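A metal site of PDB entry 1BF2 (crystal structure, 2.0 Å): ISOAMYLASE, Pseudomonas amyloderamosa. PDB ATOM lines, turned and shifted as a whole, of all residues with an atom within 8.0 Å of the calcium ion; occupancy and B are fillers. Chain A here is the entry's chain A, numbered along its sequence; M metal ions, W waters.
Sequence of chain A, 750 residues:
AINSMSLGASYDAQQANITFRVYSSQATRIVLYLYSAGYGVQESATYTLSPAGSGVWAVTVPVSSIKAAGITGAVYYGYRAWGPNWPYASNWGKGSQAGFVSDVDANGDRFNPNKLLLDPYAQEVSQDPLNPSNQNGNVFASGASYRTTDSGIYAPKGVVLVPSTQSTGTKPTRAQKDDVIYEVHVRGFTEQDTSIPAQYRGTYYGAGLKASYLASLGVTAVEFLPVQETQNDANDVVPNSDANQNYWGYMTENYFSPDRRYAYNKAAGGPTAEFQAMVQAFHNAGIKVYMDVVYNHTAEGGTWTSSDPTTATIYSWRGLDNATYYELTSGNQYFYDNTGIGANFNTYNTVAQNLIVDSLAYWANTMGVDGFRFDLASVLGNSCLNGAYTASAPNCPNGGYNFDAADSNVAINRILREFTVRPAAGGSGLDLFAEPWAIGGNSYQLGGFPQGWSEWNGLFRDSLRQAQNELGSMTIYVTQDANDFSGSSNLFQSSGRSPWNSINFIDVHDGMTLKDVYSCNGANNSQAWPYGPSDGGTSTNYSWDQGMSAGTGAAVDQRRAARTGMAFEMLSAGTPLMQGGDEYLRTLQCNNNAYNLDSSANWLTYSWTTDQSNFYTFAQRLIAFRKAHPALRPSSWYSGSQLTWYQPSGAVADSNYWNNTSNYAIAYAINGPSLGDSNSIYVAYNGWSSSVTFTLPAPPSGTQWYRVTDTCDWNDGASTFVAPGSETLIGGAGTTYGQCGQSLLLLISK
OG1 of Thr 230 is in hydrogen-bond range of O of Met 251 (2.8 Å). The side-chain hydroxyl (OG1) of Thr 230 is in hydrogen-bond range of the side-chain amide oxygen (OD1) of Asn 246 (2.9 Å). OD1 of Asp 259 is in hydrogen-bond range of N of Arg 261 (2.9 Å). The backbone NH (N) of Asp 259 lies within hydrogen-bond range of the backbone carbonyl oxygen (O) of Val 227 (2.8 Å). The side-chain carboxylate of Asp 233 sits at hydrogen-bond distance from the backbone NH of Asp 128. The side-chain carboxylate (OD1) of Asp 128 lies close to the side-chain carboxylate (OE1) of Glu 253, 2.7 Å away. N of Glu 253 lies within hydrogen-bond range of O of Glu 229, at 2.9 Å. N of Glu 229 is in hydrogen-bond range of O of Ser 257 (2.7 Å).
Five residues have an atom within 4 Å of the calcium ion: Asp 128, Glu 229, Thr 230, Asn 232 and Asp 259. The nearest printed residue that does not touch the calcium ion is Asp 233 (4.01 Å).
The calcium ion is bound by OD1 of Asn 232 (2.3 Å), O of Thr 230 (2.4 Å), water W1 (2.4 Å), OD2 of Asp 259 (2.5 Å), OD2 of Asp 128 (2.5 Å), OE1 of Glu 229 (2.5 Å) and OD1 of Asp 128 (2.6 Å).
Water W1 lies within hydrogen-bond range of OD1 of Asp 233 (2.7 Å) and N of Arg 261 (3.3 Å).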
ATOM      1  N   VAL A 125      34.259 -25.137  -6.645  1.00  0.00           N
ATOM      2  CA  VAL A 125      34.050 -25.143  -8.110  1.00  0.00           C
ATOM      3  C   VAL A 125      33.428 -23.814  -8.499  1.00  0.00           C
ATOM      4  O   VAL A 125      32.503 -23.367  -7.829  1.00  0.00           O
ATOM      5  CB  VAL A 125      33.117 -26.342  -8.538  1.00  0.00           C
ATOM      6  CG1 VAL A 125      32.840 -26.330 -10.065  1.00  0.00           C
ATOM      7  CG2 VAL A 125      33.788 -27.665  -8.180  1.00  0.00           C
ATOM      8  N   SER A 126      33.913 -23.196  -9.566  1.00  0.00           N
ATOM      9  CA  SER A 126      33.409 -21.889 -10.005  1.00  0.00           C
ATOM     10  C   SER A 126      31.964 -21.897 -10.505  1.00  0.00           C
ATOM     11  O   SER A 126      31.155 -21.051 -10.112  1.00  0.00           O
ATOM     12  CB  SER A 126      34.336 -21.269 -11.043  1.00  0.00           C
ATOM     13  OG  SER A 126      34.364 -22.053 -12.210  1.00  0.00           O
ATOM     14  N   GLN A 127      31.655 -22.817 -11.416  1.00  0.00           N
ATOM     15  CA  GLN A 127      30.300 -22.963 -11.932  1.00  0.00           C
ATOM     16  C   GLN A 127      30.167 -24.355 -12.523  1.00  0.00           C
ATOM     17  O   GLN A 127      31.173 -25.040 -12.749  1.00  0.00           O
ATOM     18  CB  GLN A 127      29.939 -21.875 -12.957  1.00  0.00           C
ATOM     19  CG  GLN A 127      30.512 -22.064 -14.356  1.00  0.00           C
ATOM     20  CD  GLN A 127      32.006 -21.801 -14.443  1.00  0.00           C
ATOM     21  OE1 GLN A 127      32.712 -22.427 -15.234  1.00  0.00           O
ATOM     22  NE2 GLN A 127      32.499 -20.853 -13.647  1.00  0.00           N
ATOM     23  N   ASP A 128      28.918 -24.800 -12.681  1.00  0.00           N
ATOM     24  CA  ASP A 128      28.637 -26.125 -13.213  1.00  0.00           C
ATOM     25  C   ASP A 128      28.769 -26.123 -14.717  1.00  0.00           C
ATOM     26  O   ASP A 128      28.708 -25.063 -15.343  1.00  0.00           O
ATOM     27  CB  ASP A 128      27.200 -26.551 -12.854  1.00  0.00           C
ATOM     28  CG  ASP A 128      26.936 -26.533 -11.367  1.00  0.00           C
ATOM     29  OD1 ASP A 128      27.855 -26.782 -10.557  1.00  0.00           O
ATOM     30  OD2 ASP A 128      25.767 -26.267 -11.012  1.00  0.00           O
ATOM     31  N   PRO A 129      28.919 -27.313 -15.310  1.00  0.00           N
ATOM     32  CA  PRO A 129      29.037 -27.418 -16.763  1.00  0.00           C
ATOM     33  C   PRO A 129      27.926 -26.626 -17.477  1.00  0.00           C
ATOM     34  O   PRO A 129      28.179 -25.872 -18.420  1.00  0.00           O
ATOM     35  CB  PRO A 129      28.914 -28.925 -16.973  1.00  0.00           C
ATOM     36  CG  PRO A 129      29.637 -29.475 -15.763  1.00  0.00           C
ATOM     37  CD  PRO A 129      29.071 -28.628 -14.663  1.00  0.00           C
ATOM     38  N   LEU A 130      26.697 -26.796 -17.004  1.00  0.00           N
ATOM     39  CA  LEU A 130      25.524 -26.114 -17.562  1.00  0.00           C
ATOM     40  C   LEU A 130      25.171 -25.011 -16.561  1.00  0.00           C
ATOM     41  O   LEU A 130      25.050 -25.244 -15.372  1.00  0.00           O
ATOM     42  CB  LEU A 130      24.357 -27.085 -17.727  1.00  0.00           C
ATOM     43  CG  LEU A 130      24.352 -27.999 -18.962  1.00  0.00           C
ATOM     44  CD1 LEU A 130      25.746 -28.361 -19.448  1.00  0.00           C
ATOM     45  CD2 LEU A 130      23.555 -29.221 -18.632  1.00  0.00           C
ATOM     46  N   VAL A 227      25.106 -32.168  -0.763  1.00  0.00           N
ATOM     47  CA  VAL A 227      25.599 -30.792  -0.754  1.00  0.00           C
ATOM     48  C   VAL A 227      26.920 -30.676  -1.528  1.00  0.00           C
ATOM     49  O   VAL A 227      27.427 -29.569  -1.774  1.00  0.00           O
ATOM     50  CB  VAL A 227      25.740 -30.176   0.684  1.00  0.00           C
ATOM     51  CG1 VAL A 227      24.355 -29.829   1.259  1.00  0.00           C
ATOM     52  CG2 VAL A 227      26.448 -31.131   1.604  1.00  0.00           C
ATOM     53  N   GLN A 228      27.502 -31.809  -1.884  1.00  0.00           N
ATOM     54  CA  GLN A 228      28.717 -31.759  -2.682  1.00  0.00           C
ATOM     55  C   GLN A 228      28.239 -31.298  -4.058  1.00  0.00           C
ATOM     56  O   GLN A 228      27.193 -31.756  -4.530  1.00  0.00           O
ATOM     57  CB  GLN A 228      29.373 -33.132  -2.775  1.00  0.00           C
ATOM     58  CG  GLN A 228      30.084 -33.564  -1.496  1.00  0.00           C
ATOM     59  CD  GLN A 228      30.263 -35.066  -1.397  1.00  0.00           C
ATOM     60  OE1 GLN A 228      29.404 -35.823  -1.801  1.00  0.00           O
ATOM     61  NE2 GLN A 228      31.374 -35.494  -0.857  1.00  0.00           N
ATOM     62  N   GLU A 229      28.954 -30.348  -4.653  1.00  0.00           N
ATOM     63  CA  GLU A 229      28.617 -29.798  -5.973  1.00  0.00           C
ATOM     64  C   GLU A 229      27.845 -30.693  -6.913  1.00  0.00           C
ATOM     65  O   GLU A 229      28.320 -31.759  -7.299  1.00  0.00           O
ATOM     66  CB  GLU A 229      29.885 -29.349  -6.720  1.00  0.00           C
ATOM     67  CG  GLU A 229      30.386 -27.972  -6.369  1.00  0.00           C
ATOM     68  CD  GLU A 229      29.512 -26.859  -6.906  1.00  0.00           C
ATOM     69  OE1 GLU A 229      28.515 -27.159  -7.598  1.00  0.00           O
ATOM     70  OE2 GLU A 229      29.821 -25.678  -6.648  1.00  0.00           O
ATOM     71  N   THR A 230      26.671 -30.237  -7.327  1.00  0.00           N
ATOM     72  CA  THR A 230      25.864 -30.981  -8.285  1.00  0.00           C
ATOM     73  C   THR A 230      25.490 -30.041  -9.433  1.00  0.00           C
ATOM     74  O   THR A 230      25.695 -28.817  -9.341  1.00  0.00           O
ATOM     75  CB  THR A 230      24.610 -31.591  -7.621  1.00  0.00           C
ATOM     76  OG1 THR A 230      23.965 -32.503  -8.514  1.00  0.00           O
ATOM     77  CG2 THR A 230      23.641 -30.505  -7.183  1.00  0.00           C
ATOM     78  N   GLN A 231      25.028 -30.616 -10.532  1.00  0.00           N
ATOM     79  CA  GLN A 231      24.599 -29.872 -11.704  1.00  0.00           C
ATOM     80  C   GLN A 231      23.247 -29.216 -11.392  1.00  0.00           C
ATOM     81  O   GLN A 231      22.211 -29.884 -11.438  1.00  0.00           O
ATOM     82  CB  GLN A 231      24.457 -30.806 -12.917  1.00  0.00           C
ATOM     83  CG  GLN A 231      23.851 -30.147 -14.159  1.00  0.00           C
ATOM     84  CD  GLN A 231      24.628 -28.905 -14.594  1.00  0.00           C
ATOM     85  OE1 GLN A 231      24.151 -27.774 -14.409  1.00  0.00           O
ATOM     86  NE2 GLN A 231      25.824 -29.105 -15.146  1.00  0.00           N
ATOM     87  N   ASN A 232      23.269 -27.924 -11.094  1.00  0.00           N
ATOM     88  CA  ASN A 232      22.042 -27.199 -10.769  1.00  0.00           C
ATOM     89  C   ASN A 232      22.006 -25.713 -11.167  1.00  0.00           C
ATOM     90  O   ASN A 232      20.948 -25.091 -11.087  1.00  0.00           O
ATOM     91  CB  ASN A 232      21.702 -27.368  -9.276  1.00  0.00           C
ATOM     92  CG  ASN A 232      22.836 -26.954  -8.329  1.00  0.00           C
ATOM     93  OD1 ASN A 232      23.903 -26.456  -8.754  1.00  0.00           O
ATOM     94  ND2 ASN A 232      22.636 -27.195  -7.052  1.00  0.00           N
ATOM     95  N   ASP A 233      23.117 -25.160 -11.641  1.00  0.00           N
ATOM     96  CA  ASP A 233      23.147 -23.742 -12.043  1.00  0.00           C
ATOM     97  C   ASP A 233      22.231 -23.348 -13.209  1.00  0.00           C
ATOM     98  O   ASP A 233      21.960 -22.164 -13.394  1.00  0.00           O
ATOM     99  CB  ASP A 233      24.579 -23.291 -12.365  1.00  0.00           C
ATOM    100  CG  ASP A 233      25.447 -23.162 -11.118  1.00  0.00           C
ATOM    101  OD1 ASP A 233      24.920 -23.138  -9.987  1.00  0.00           O
ATOM    102  OD2 ASP A 233      26.673 -23.064 -11.287  1.00  0.00           O
ATOM    103  N   ALA A 234      21.794 -24.308 -14.021  1.00  0.00           N
ATOM    104  CA  ALA A 234      20.925 -23.989 -15.154  1.00  0.00           C
ATOM    105  C   ALA A 234      19.467 -24.308 -14.836  1.00  0.00           C
ATOM    106  O   ALA A 234      18.613 -24.269 -15.731  1.00  0.00           O
ATOM    107  CB  ALA A 234      21.360 -24.759 -16.417  1.00  0.00           C
ATOM    108  N   ASN A 246      17.615 -30.401 -11.900  1.00  0.00           N
ATOM    109  CA  ASN A 246      18.154 -31.457 -11.060  1.00  0.00           C
ATOM    110  C   ASN A 246      18.015 -30.844  -9.683  1.00  0.00           C
ATOM    111  O   ASN A 246      18.718 -29.897  -9.352  1.00  0.00           O
ATOM    112  CB  ASN A 246      19.627 -31.721 -11.395  1.00  0.00           C
ATOM    113  CG  ASN A 246      20.319 -32.603 -10.341  1.00  0.00           C
ATOM    114  OD1 ASN A 246      21.519 -32.453 -10.092  1.00  0.00           O
ATOM    115  ND2 ASN A 246      19.574 -33.530  -9.744  1.00  0.00           N
ATOM    116  N   MET A 251      24.150 -36.333  -8.505  1.00  0.00           N
ATOM    117  CA  MET A 251      25.068 -36.292  -9.642  1.00  0.00           C
ATOM    118  C   MET A 251      26.164 -35.398  -9.118  1.00  0.00           C
ATOM    119  O   MET A 251      26.063 -34.184  -9.196  1.00  0.00           O
ATOM    120  CB  MET A 251      24.414 -35.611 -10.857  1.00  0.00           C
ATOM    121  CG  MET A 251      23.311 -36.407 -11.496  1.00  0.00           C
ATOM    122  SD  MET A 251      23.929 -37.989 -12.075  1.00  0.00           S
ATOM    123  CE  MET A 251      24.207 -37.662 -13.738  1.00  0.00           C
ATOM    124  N   GLU A 253      29.696 -33.606  -9.015  1.00  0.00           N
ATOM    125  CA  GLU A 253      30.713 -33.106  -9.939  1.00  0.00           C
ATOM    126  C   GLU A 253      32.080 -33.061  -9.300  1.00  0.00           C
ATOM    127  O   GLU A 253      33.089 -33.024 -10.002  1.00  0.00           O
ATOM    128  CB  GLU A 253      30.363 -31.684 -10.371  1.00  0.00           C
ATOM    129  CG  GLU A 253      28.940 -31.503 -10.842  1.00  0.00           C
ATOM    130  CD  GLU A 253      28.607 -30.064 -11.168  1.00  0.00           C
ATOM    131  OE1 GLU A 253      29.161 -29.156 -10.500  1.00  0.00           O
ATOM    132  OE2 GLU A 253      27.773 -29.852 -12.072  1.00  0.00           O
ATOM    133  N   SER A 257      33.782 -30.140  -2.727  1.00  0.00           N
ATOM    134  CA  SER A 257      33.166 -28.816  -2.825  1.00  0.00           C
ATOM    135  C   SER A 257      31.709 -28.656  -2.458  1.00  0.00           C
ATOM    136  O   SER A 257      30.860 -29.395  -2.963  1.00  0.00           O
ATOM    137  CB  SER A 257      33.341 -28.285  -4.245  1.00  0.00           C
ATOM    138  OG  SER A 257      34.708 -28.305  -4.657  1.00  0.00           O
ATOM    139  N   PRO A 258      31.395 -27.652  -1.614  1.00  0.00           N
ATOM    140  CA  PRO A 258      30.015 -27.399  -1.209  1.00  0.00           C
ATOM    141  C   PRO A 258      29.408 -26.765  -2.433  1.00  0.00           C
ATOM    142  O   PRO A 258      30.080 -25.986  -3.102  1.00  0.00           O
ATOM    143  CB  PRO A 258      30.161 -26.347  -0.111  1.00  0.00           C
ATOM    144  CG  PRO A 258      31.617 -26.392   0.279  1.00  0.00           C
ATOM    145  CD  PRO A 258      32.292 -26.652  -1.012  1.00  0.00           C
ATOM    146  N   ASP A 259      28.165 -27.088  -2.732  1.00  0.00           N
ATOM    147  CA  ASP A 259      27.510 -26.531  -3.898  1.00  0.00           C
ATOM    148  C   ASP A 259      27.350 -25.031  -3.762  1.00  0.00           C
ATOM    149  O   ASP A 259      26.788 -24.547  -2.801  1.00  0.00           O
ATOM    150  CB  ASP A 259      26.144 -27.178  -4.078  1.00  0.00           C
ATOM    151  CG  ASP A 259      25.539 -26.869  -5.404  1.00  0.00           C
ATOM    152  OD1 ASP A 259      24.881 -25.831  -5.537  1.00  0.00           O
ATOM    153  OD2 ASP A 259      25.733 -27.663  -6.326  1.00  0.00           O
ATOM    154  N   ARG A 260      27.812 -24.320  -4.771  1.00  0.00           N
ATOM    155  CA  ARG A 260      27.782 -22.867  -4.799  1.00  0.00           C
ATOM    156  C   ARG A 260      26.367 -22.287  -4.877  1.00  0.00           C
ATOM    157  O   ARG A 260      26.082 -21.232  -4.285  1.00  0.00           O
ATOM    158  CB  ARG A 260      28.618 -22.415  -5.989  1.00  0.00           C
ATOM    159  CG  ARG A 260      28.940 -20.959  -6.041  1.00  0.00           C
ATOM    160  CD  ARG A 260      30.199 -20.755  -6.858  1.00  0.00           C
ATOM    161  NE  ARG A 260      31.104 -19.996  -6.024  1.00  0.00           N
ATOM    162  CZ  ARG A 260      32.221 -20.448  -5.482  1.00  0.00           C
ATOM    163  NH1 ARG A 260      32.639 -21.675  -5.669  1.00  0.00           N
ATOM    164  NH2 ARG A 260      32.822 -19.711  -4.576  1.00  0.00           N
ATOM    165  N   ARG A 261      25.473 -22.965  -5.569  1.00  0.00           N
ATOM    166  CA  ARG A 261      24.098 -22.483  -5.705  1.00  0.00           C
ATOM    167  C   ARG A 261      23.339 -22.442  -4.388  1.00  0.00           C
ATOM    168  O   ARG A 261      22.367 -21.715  -4.258  1.00  0.00           O
ATOM    169  CB  ARG A 261      23.335 -23.341  -6.714  1.00  0.00           C
ATOM    170  CG  ARG A 261      21.855 -23.069  -6.794  1.00  0.00           C
ATOM    171  CD  ARG A 261      21.268 -23.907  -7.890  1.00  0.00           C
ATOM    172  NE  ARG A 261      19.804 -23.906  -7.904  1.00  0.00           N
ATOM    173  CZ  ARG A 261      19.069 -23.111  -8.681  1.00  0.00           C
ATOM    174  NH1 ARG A 261      19.667 -22.243  -9.484  1.00  0.00           N
ATOM    175  NH2 ARG A 261      17.762 -23.240  -8.729  1.00  0.00           N
ATOM    176  N   TYR A 262      23.773 -23.232  -3.420  1.00  0.00           N
ATOM    177  CA  TYR A 262      23.110 -23.306  -2.129  1.00  0.00           C
ATOM    178  C   TYR A 262      23.710 -22.342  -1.114  1.00  0.00           C
ATOM    179  O   TYR A 262      23.276 -22.301   0.047  1.00  0.00           O
ATOM    180  CB  TYR A 262      23.218 -24.724  -1.558  1.00  0.00           C
ATOM    181  CG  TYR A 262      22.572 -25.854  -2.357  1.00  0.00           C
ATOM    182  CD1 TYR A 262      21.510 -25.626  -3.228  1.00  0.00           C
ATOM    183  CD2 TYR A 262      22.992 -27.156  -2.171  1.00  0.00           C
ATOM    184  CE1 TYR A 262      20.870 -26.690  -3.887  1.00  0.00           C
ATOM    185  CE2 TYR A 262      22.370 -28.219  -2.817  1.00  0.00           C
ATOM    186  CZ  TYR A 262      21.315 -27.988  -3.666  1.00  0.00           C
ATOM    187  OH  TYR A 262      20.725 -29.092  -4.283  1.00  0.00           O
HETATM  188 CA    CA M   1      26.207 -26.651  -8.555  1.00  0.00          CA
HETATM  189  O   HOH W   1      26.639 -24.335  -8.314  1.00  0.00           O
